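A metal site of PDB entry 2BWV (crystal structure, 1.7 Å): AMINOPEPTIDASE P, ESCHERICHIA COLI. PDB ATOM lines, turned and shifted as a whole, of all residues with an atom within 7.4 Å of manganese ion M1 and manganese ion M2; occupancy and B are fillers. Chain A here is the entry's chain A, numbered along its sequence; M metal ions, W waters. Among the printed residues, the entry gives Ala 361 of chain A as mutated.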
ATOM      1  N   TYR A 229      -3.329  15.916   2.689  1.00  0.00           N
ATOM      2  CA  TYR A 229      -3.364  14.628   1.996  1.00  0.00           C
ATOM      3  C   TYR A 229      -3.954  13.622   2.976  1.00  0.00           C
ATOM      4  O   TYR A 229      -4.060  13.898   4.156  1.00  0.00           O
ATOM      5  CB  TYR A 229      -1.983  14.170   1.550  1.00  0.00           C
ATOM      6  CG  TYR A 229      -0.978  14.151   2.665  1.00  0.00           C
ATOM      7  CD1 TYR A 229      -0.259  15.300   2.972  1.00  0.00           C
ATOM      8  CD2 TYR A 229      -0.753  13.002   3.450  1.00  0.00           C
ATOM      9  CE1 TYR A 229       0.651  15.317   4.024  1.00  0.00           C
ATOM     10  CE2 TYR A 229       0.179  13.008   4.501  1.00  0.00           C
ATOM     11  CZ  TYR A 229       0.884  14.168   4.777  1.00  0.00           C
ATOM     12  OH  TYR A 229       1.805  14.241   5.783  1.00  0.00           O
ATOM     13  N   ILE A 232      -1.900   8.788   6.871  1.00  0.00           N
ATOM     14  CA  ILE A 232      -1.370   7.420   6.903  1.00  0.00           C
ATOM     15  C   ILE A 232      -1.012   7.066   8.368  1.00  0.00           C
ATOM     16  O   ILE A 232      -0.216   7.756   9.004  1.00  0.00           O
ATOM     17  CB  ILE A 232      -0.075   7.354   6.046  1.00  0.00           C
ATOM     18  CG1 ILE A 232      -0.413   7.588   4.563  1.00  0.00           C
ATOM     19  CG2 ILE A 232       0.687   6.049   6.270  1.00  0.00           C
ATOM     20  CD1 ILE A 232       0.734   8.125   3.744  1.00  0.00           C
ATOM     21  N   ILE A 259       3.305   7.282  11.193  1.00  0.00           N
ATOM     22  CA  ILE A 259       2.259   8.263  10.945  1.00  0.00           C
ATOM     23  C   ILE A 259       2.796   9.300   9.971  1.00  0.00           C
ATOM     24  O   ILE A 259       3.794   9.993  10.266  1.00  0.00           O
ATOM     25  CB  ILE A 259       1.772   8.944  12.227  1.00  0.00           C
ATOM     26  CG1 ILE A 259       1.219   7.911  13.206  1.00  0.00           C
ATOM     27  CG2 ILE A 259       0.708   9.961  11.900  1.00  0.00           C
ATOM     28  CD1 ILE A 259       0.631   8.535  14.459  1.00  0.00           C
ATOM     29  N   ASP A 260       2.158   9.378   8.811  1.00  0.00           N
ATOM     30  CA  ASP A 260       2.484  10.394   7.810  1.00  0.00           C
ATOM     31  C   ASP A 260       1.224  11.258   7.669  1.00  0.00           C
ATOM     32  O   ASP A 260       0.177  10.781   7.236  1.00  0.00           O
ATOM     33  CB  ASP A 260       2.862   9.737   6.490  1.00  0.00           C
ATOM     34  CG  ASP A 260       3.528  10.720   5.527  1.00  0.00           C
ATOM     35  OD1 ASP A 260       3.410  11.953   5.690  1.00  0.00           O
ATOM     36  OD2 ASP A 260       4.210  10.237   4.591  1.00  0.00           O
ATOM     37  N   ALA A 261       1.312  12.478   8.192  1.00  0.00           N
ATOM     38  CA  ALA A 261       0.147  13.385   8.268  1.00  0.00           C
ATOM     39  C   ALA A 261       0.575  14.833   8.205  1.00  0.00           C
ATOM     40  O   ALA A 261       1.624  15.221   8.750  1.00  0.00           O
ATOM     41  CB  ALA A 261      -0.647  13.154   9.566  1.00  0.00           C
ATOM     42  N   GLY A 262      -0.254  15.629   7.551  1.00  0.00           N
ATOM     43  CA  GLY A 262       0.018  17.044   7.344  1.00  0.00           C
ATOM     44  C   GLY A 262      -1.253  17.857   7.191  1.00  0.00           C
ATOM     45  O   GLY A 262      -2.237  17.402   6.615  1.00  0.00           O
ATOM     46  N   GLY A 270       1.589  21.231   5.382  1.00  0.00           N
ATOM     47  CA  GLY A 270       2.598  20.583   6.199  1.00  0.00           C
ATOM     48  C   GLY A 270       2.678  19.120   5.764  1.00  0.00           C
ATOM     49  O   GLY A 270       1.771  18.588   5.106  1.00  0.00           O
ATOM     50  N   ASP A 271       3.766  18.459   6.141  1.00  0.00           N
ATOM     51  CA  ASP A 271       3.974  17.088   5.748  1.00  0.00           C
ATOM     52  C   ASP A 271       5.029  16.451   6.650  1.00  0.00           C
ATOM     53  O   ASP A 271       6.216  16.577   6.412  1.00  0.00           O
ATOM     54  CB  ASP A 271       4.353  17.040   4.273  1.00  0.00           C
ATOM     55  CG  ASP A 271       4.606  15.634   3.748  1.00  0.00           C
ATOM     56  OD1 ASP A 271       4.388  14.630   4.440  1.00  0.00           O
ATOM     57  OD2 ASP A 271       5.015  15.534   2.576  1.00  0.00           O
ATOM     58  N   ILE A 272       4.582  15.774   7.698  1.00  0.00           N
ATOM     59  CA  ILE A 272       5.499  15.173   8.664  1.00  0.00           C
ATOM     60  C   ILE A 272       5.254  13.663   8.720  1.00  0.00           C
ATOM     61  O   ILE A 272       4.096  13.195   8.676  1.00  0.00           O
ATOM     62  CB  ILE A 272       5.313  15.778  10.087  1.00  0.00           C
ATOM     63  CG1 ILE A 272       5.791  17.241  10.153  1.00  0.00           C
ATOM     64  CG2 ILE A 272       6.000  14.925  11.166  1.00  0.00           C
ATOM     65  CD1 ILE A 272       5.553  17.882  11.524  1.00  0.00           C
ATOM     66  N   THR A 273       6.336  12.911   8.844  1.00  0.00           N
ATOM     67  CA  THR A 273       6.256  11.492   9.224  1.00  0.00           C
ATOM     68  C   THR A 273       7.075  11.276  10.514  1.00  0.00           C
ATOM     69  O   THR A 273       8.212  11.757  10.650  1.00  0.00           O
ATOM     70  CB  THR A 273       6.748  10.500   8.136  1.00  0.00           C
ATOM     71  OG1 THR A 273       6.158  10.793   6.862  1.00  0.00           O
ATOM     72  CG2 THR A 273       6.426   9.028   8.530  1.00  0.00           C
ATOM     73  N   LEU A 352      14.033  10.804  -1.616  1.00  0.00           N
ATOM     74  CA  LEU A 352      14.350  11.412  -0.327  1.00  0.00           C
ATOM     75  C   LEU A 352      13.542  12.700  -0.068  1.00  0.00           C
ATOM     76  O   LEU A 352      13.281  13.073   1.086  1.00  0.00           O
ATOM     77  CB  LEU A 352      15.840  11.797  -0.302  1.00  0.00           C
ATOM     78  CG  LEU A 352      16.379  12.412   1.001  1.00  0.00           C
ATOM     79  CD1 LEU A 352      16.275  11.434   2.171  1.00  0.00           C
ATOM     80  CD2 LEU A 352      17.824  12.863   0.780  1.00  0.00           C
ATOM     81  N   SER A 353      13.195  13.402  -1.142  1.00  0.00           N
ATOM     82  CA  SER A 353      12.654  14.751  -1.031  1.00  0.00           C
ATOM     83  C   SER A 353      11.725  15.098  -2.162  1.00  0.00           C
ATOM     84  O   SER A 353      12.001  14.768  -3.321  1.00  0.00           O
ATOM     85  CB  SER A 353      13.801  15.784  -1.034  1.00  0.00           C
ATOM     86  OG  SER A 353      14.635  15.626   0.096  1.00  0.00           O
ATOM     87  N   HIS A 354      10.658  15.804  -1.819  1.00  0.00           N
ATOM     88  CA  HIS A 354       9.837  16.473  -2.818  1.00  0.00           C
ATOM     89  C   HIS A 354       9.596  17.917  -2.411  1.00  0.00           C
ATOM     90  O   HIS A 354       9.607  18.257  -1.234  1.00  0.00           O
ATOM     91  CB  HIS A 354       8.505  15.756  -3.021  1.00  0.00           C
ATOM     92  CG  HIS A 354       7.674  15.634  -1.784  1.00  0.00           C
ATOM     93  ND1 HIS A 354       6.856  16.646  -1.326  1.00  0.00           N
ATOM     94  CD2 HIS A 354       7.551  14.618  -0.906  1.00  0.00           C
ATOM     95  CE1 HIS A 354       6.263  16.250  -0.208  1.00  0.00           C
ATOM     96  NE2 HIS A 354       6.676  15.026   0.078  1.00  0.00           N
ATOM     97  N   TRP A 355       9.371  18.758  -3.410  1.00  0.00           N
ATOM     98  CA  TRP A 355       8.935  20.134  -3.163  1.00  0.00           C
ATOM     99  C   TRP A 355       7.647  20.170  -2.335  1.00  0.00           C
ATOM    100  O   TRP A 355       6.827  19.238  -2.395  1.00  0.00           O
ATOM    101  CB  TRP A 355       8.657  20.879  -4.469  1.00  0.00           C
ATOM    102  CG  TRP A 355       9.705  20.824  -5.548  1.00  0.00           C
ATOM    103  CD1 TRP A 355       9.495  20.506  -6.861  1.00  0.00           C
ATOM    104  CD2 TRP A 355      11.101  21.167  -5.434  1.00  0.00           C
ATOM    105  NE1 TRP A 355      10.666  20.601  -7.564  1.00  0.00           N
ATOM    106  CE2 TRP A 355      11.677  21.001  -6.728  1.00  0.00           C
ATOM    107  CE3 TRP A 355      11.925  21.580  -4.387  1.00  0.00           C
ATOM    108  CZ2 TRP A 355      13.028  21.253  -7.011  1.00  0.00           C
ATOM    109  CZ3 TRP A 355      13.296  21.826  -4.663  1.00  0.00           C
ATOM    110  CH2 TRP A 355      13.823  21.654  -5.965  1.00  0.00           C
ATOM    111  N   LEU A 356       7.453  21.253  -1.596  1.00  0.00           N
ATOM    112  CA  LEU A 356       6.310  21.413  -0.703  1.00  0.00           C
ATOM    113  C   LEU A 356       5.727  22.828  -0.883  1.00  0.00           C
ATOM    114  O   LEU A 356       6.473  23.802  -0.973  1.00  0.00           O
ATOM    115  CB  LEU A 356       6.749  21.211   0.753  1.00  0.00           C
ATOM    116  CG  LEU A 356       5.707  21.266   1.868  1.00  0.00           C
ATOM    117  CD1 LEU A 356       4.715  20.105   1.764  1.00  0.00           C
ATOM    118  CD2 LEU A 356       6.389  21.258   3.242  1.00  0.00           C
ATOM    119  N   VAL A 360       1.056  19.245  -1.551  1.00  0.00           N
ATOM    120  CA  VAL A 360       2.017  18.527  -0.746  1.00  0.00           C
ATOM    121  C   VAL A 360       3.176  18.018  -1.581  1.00  0.00           C
ATOM    122  O   VAL A 360       4.325  18.195  -1.184  1.00  0.00           O
ATOM    123  CB  VAL A 360       1.382  17.400   0.146  1.00  0.00           C
ATOM    124  CG1 VAL A 360       0.701  16.366  -0.671  1.00  0.00           C
ATOM    125  CG2 VAL A 360       2.448  16.815   1.060  1.00  0.00           C
ATOM    126  N   ALA A 361       2.882  17.396  -2.722  1.00  0.00           N
ATOM    127  CA  ALA A 361       3.926  17.068  -3.716  1.00  0.00           C
ATOM    128  C   ALA A 361       3.909  18.239  -4.712  1.00  0.00           C
ATOM    129  O   ALA A 361       3.188  18.224  -5.734  1.00  0.00           O
ATOM    130  CB  ALA A 361       3.653  15.754  -4.384  1.00  0.00           C
ATOM    131  N   LEU A 380      11.105  22.001   0.683  1.00  0.00           N
ATOM    132  CA  LEU A 380      11.108  20.573   0.360  1.00  0.00           C
ATOM    133  C   LEU A 380      11.049  19.717   1.619  1.00  0.00           C
ATOM    134  O   LEU A 380      11.332  20.176   2.744  1.00  0.00           O
ATOM    135  CB  LEU A 380      12.316  20.175  -0.494  1.00  0.00           C
ATOM    136  CG  LEU A 380      13.739  20.411   0.097  1.00  0.00           C
ATOM    137  CD1 LEU A 380      14.798  19.438  -0.460  1.00  0.00           C
ATOM    138  CD2 LEU A 380      14.208  21.864  -0.084  1.00  0.00           C
ATOM    139  N   THR A 381      10.648  18.463   1.413  1.00  0.00           N
ATOM    140  CA  THR A 381      10.652  17.511   2.494  1.00  0.00           C
ATOM    141  C   THR A 381      11.971  16.743   2.534  1.00  0.00           C
ATOM    142  O   THR A 381      12.720  16.734   1.557  1.00  0.00           O
ATOM    143  CB  THR A 381       9.510  16.487   2.347  1.00  0.00           C
ATOM    144  OG1 THR A 381       9.747  15.700   1.170  1.00  0.00           O
ATOM    145  CG2 THR A 381       8.145  17.174   2.255  1.00  0.00           C
ATOM    146  N   VAL A 382      12.228  16.077   3.650  1.00  0.00           N
ATOM    147  CA  VAL A 382      13.366  15.168   3.784  1.00  0.00           C
ATOM    148  C   VAL A 382      12.818  13.947   4.492  1.00  0.00           C
ATOM    149  O   VAL A 382      12.439  14.026   5.658  1.00  0.00           O
ATOM    150  CB  VAL A 382      14.529  15.802   4.588  1.00  0.00           C
ATOM    151  CG1 VAL A 382      15.781  14.910   4.547  1.00  0.00           C
ATOM    152  CG2 VAL A 382      14.831  17.226   4.066  1.00  0.00           C
ATOM    153  N   GLU A 383      12.715  12.830   3.780  1.00  0.00           N
ATOM    154  CA  GLU A 383      11.938  11.676   4.255  1.00  0.00           C
ATOM    155  C   GLU A 383      12.570  10.320   3.942  1.00  0.00           C
ATOM    156  O   GLU A 383      11.974   9.477   3.257  1.00  0.00           O
ATOM    157  CB  GLU A 383      10.493  11.763   3.754  1.00  0.00           C
ATOM    158  CG  GLU A 383      10.299  11.781   2.273  1.00  0.00           C
ATOM    159  CD  GLU A 383       8.840  12.033   1.960  1.00  0.00           C
ATOM    160  OE1 GLU A 383       7.977  11.223   2.398  1.00  0.00           O
ATOM    161  OE2 GLU A 383       8.559  13.061   1.322  1.00  0.00           O
ATOM    162  N   ARG A 404       9.741   5.501   8.578  1.00  0.00           N
ATOM    163  CA  ARG A 404      10.063   6.723   7.874  1.00  0.00           C
ATOM    164  C   ARG A 404      10.073   7.882   8.861  1.00  0.00           C
ATOM    165  O   ARG A 404       9.267   7.919   9.801  1.00  0.00           O
ATOM    166  CB  ARG A 404       9.074   6.966   6.723  1.00  0.00           C
ATOM    167  CG  ARG A 404       9.219   8.284   6.000  1.00  0.00           C
ATOM    168  CD  ARG A 404       8.485   8.313   4.660  1.00  0.00           C
ATOM    169  NE  ARG A 404       7.025   8.353   4.755  1.00  0.00           N
ATOM    170  CZ  ARG A 404       6.184   7.325   4.566  1.00  0.00           C
ATOM    171  NH1 ARG A 404       6.638   6.111   4.302  1.00  0.00           N
ATOM    172  NH2 ARG A 404       4.865   7.479   4.650  1.00  0.00           N
ATOM    173  N   GLU A 406      10.261  12.164   8.607  1.00  0.00           N
ATOM    174  CA  GLU A 406      10.151  13.210   7.604  1.00  0.00           C
ATOM    175  C   GLU A 406       9.983  14.583   8.232  1.00  0.00           C
ATOM    176  O   GLU A 406       9.091  14.779   9.075  1.00  0.00           O
ATOM    177  CB  GLU A 406       8.986  12.912   6.683  1.00  0.00           C
ATOM    178  CG  GLU A 406       8.597  14.055   5.760  1.00  0.00           C
ATOM    179  CD  GLU A 406       7.482  13.677   4.810  1.00  0.00           C
ATOM    180  OE1 GLU A 406       6.644  12.799   5.139  1.00  0.00           O
ATOM    181  OE2 GLU A 406       7.458  14.261   3.720  1.00  0.00           O
ATOM    182  N   ASP A 407      10.843  15.525   7.809  1.00  0.00           N
ATOM    183  CA  ASP A 407      10.746  16.950   8.191  1.00  0.00           C
ATOM    184  C   ASP A 407      10.553  17.792   6.926  1.00  0.00           C
ATOM    185  O   ASP A 407      10.814  17.331   5.803  1.00  0.00           O
ATOM    186  CB  ASP A 407      12.003  17.416   8.938  1.00  0.00           C
ATOM    187  CG  ASP A 407      12.006  17.032  10.427  1.00  0.00           C
ATOM    188  OD1 ASP A 407      10.900  16.856  11.036  1.00  0.00           O
ATOM    189  OD2 ASP A 407      13.129  16.913  10.971  1.00  0.00           O
ATOM    190  N   ASP A 408      10.051  19.016   7.117  1.00  0.00           N
ATOM    191  CA  ASP A 408       9.877  20.000   6.049  1.00  0.00           C
ATOM    192  C   ASP A 408      10.896  21.109   6.286  1.00  0.00           C
ATOM    193  O   ASP A 408      11.032  21.603   7.418  1.00  0.00           O
ATOM    194  CB  ASP A 408       8.466  20.574   6.058  1.00  0.00           C
ATOM    195  CG  ASP A 408       7.406  19.485   6.063  1.00  0.00           C
ATOM    196  OD1 ASP A 408       7.709  18.415   5.479  1.00  0.00           O
ATOM    197  OD2 ASP A 408       6.325  19.713   6.655  1.00  0.00           O
HETATM  198 MN    MN M   1       4.816  12.659   4.068  1.00  0.00          MN
HETATM  199 MN    MN M   2       6.464  14.058   1.967  1.00  0.00          MN
HETATM  200  O   HOH W   1       5.518  12.301   2.261  1.00  0.00           O
HETATM  201  O   HOH W   2       2.786  12.602   2.616  1.00  0.00           O
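Manganese ion M1 is bound by water W1, the side-chain carboxylate (OD1) of Asp 271, the side-chain carboxylate (OE1) of Glu 406, the side-chain carboxylate (OD1) of Asp 260, water W2 and the side-chain carboxylate (OD2) of Asp 260.
Residues that only touch manganese ion M2: Thr 381 (3.6 Å). Five residues have an atom within 4 Å of manganese ion M2: Asp 271, His 354, Thr 381, Glu 383 and Glu 406. The nearest printed residue that does not touch manganese ion M2 is Val 360 (5.0 Å).
Water W1 binds manganese ion M2, at 2.0 Å. OE2 of Glu 406 is bound to manganese ion M2 (2.0 Å). Manganese ion M2 is bound by NE2 of His 354 (2.1 Å). OD2 of Asp 271 is bound to manganese ion M2. OE2 of Glu 383 binds manganese ion M2. Manganese ion M2 has five donor atoms within binding distance.
The side-chain carboxylate (OD2) of Asp 260 sits close to the side-chain hydroxyl (OG1) of Thr 273. The backbone carbonyl oxygen (O) of Thr 273 sits at hydrogen-bond distance from the backbone NH (N) of Glu 406, 2.9 Å away. OH of Tyr 229 lies close to OD1 of Asp 271 (2.9 Å). OE2 of Glu 383 sits close to OG1 of Thr 381, at 2.9 Å. OD2 of Asp 260 lies close to NH2 of Arg 404, 2.8 Å away. The side-chain hydroxyl of Ser 353 lies within hydrogen-bond range of the backbone carbonyl oxygen of Thr 381, at 2.7 Å. OG1 of Thr 273 is in hydrogen-bond range of NE of Arg 404 (3.3 Å). O of Val 360 sits close to ND1 of His 354 (3.0 Å).
Merely in contact with manganese ion M1: Thr 273 and Tyr 229. Six residues have an atom within 4 Å of manganese ion M1: Tyr 229, Asp 260, Asp 271, Thr 273, Glu 383 and Glu 406. The nearest printed residue that does not touch manganese ion M1 is Ile 272 (4.7 Å).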
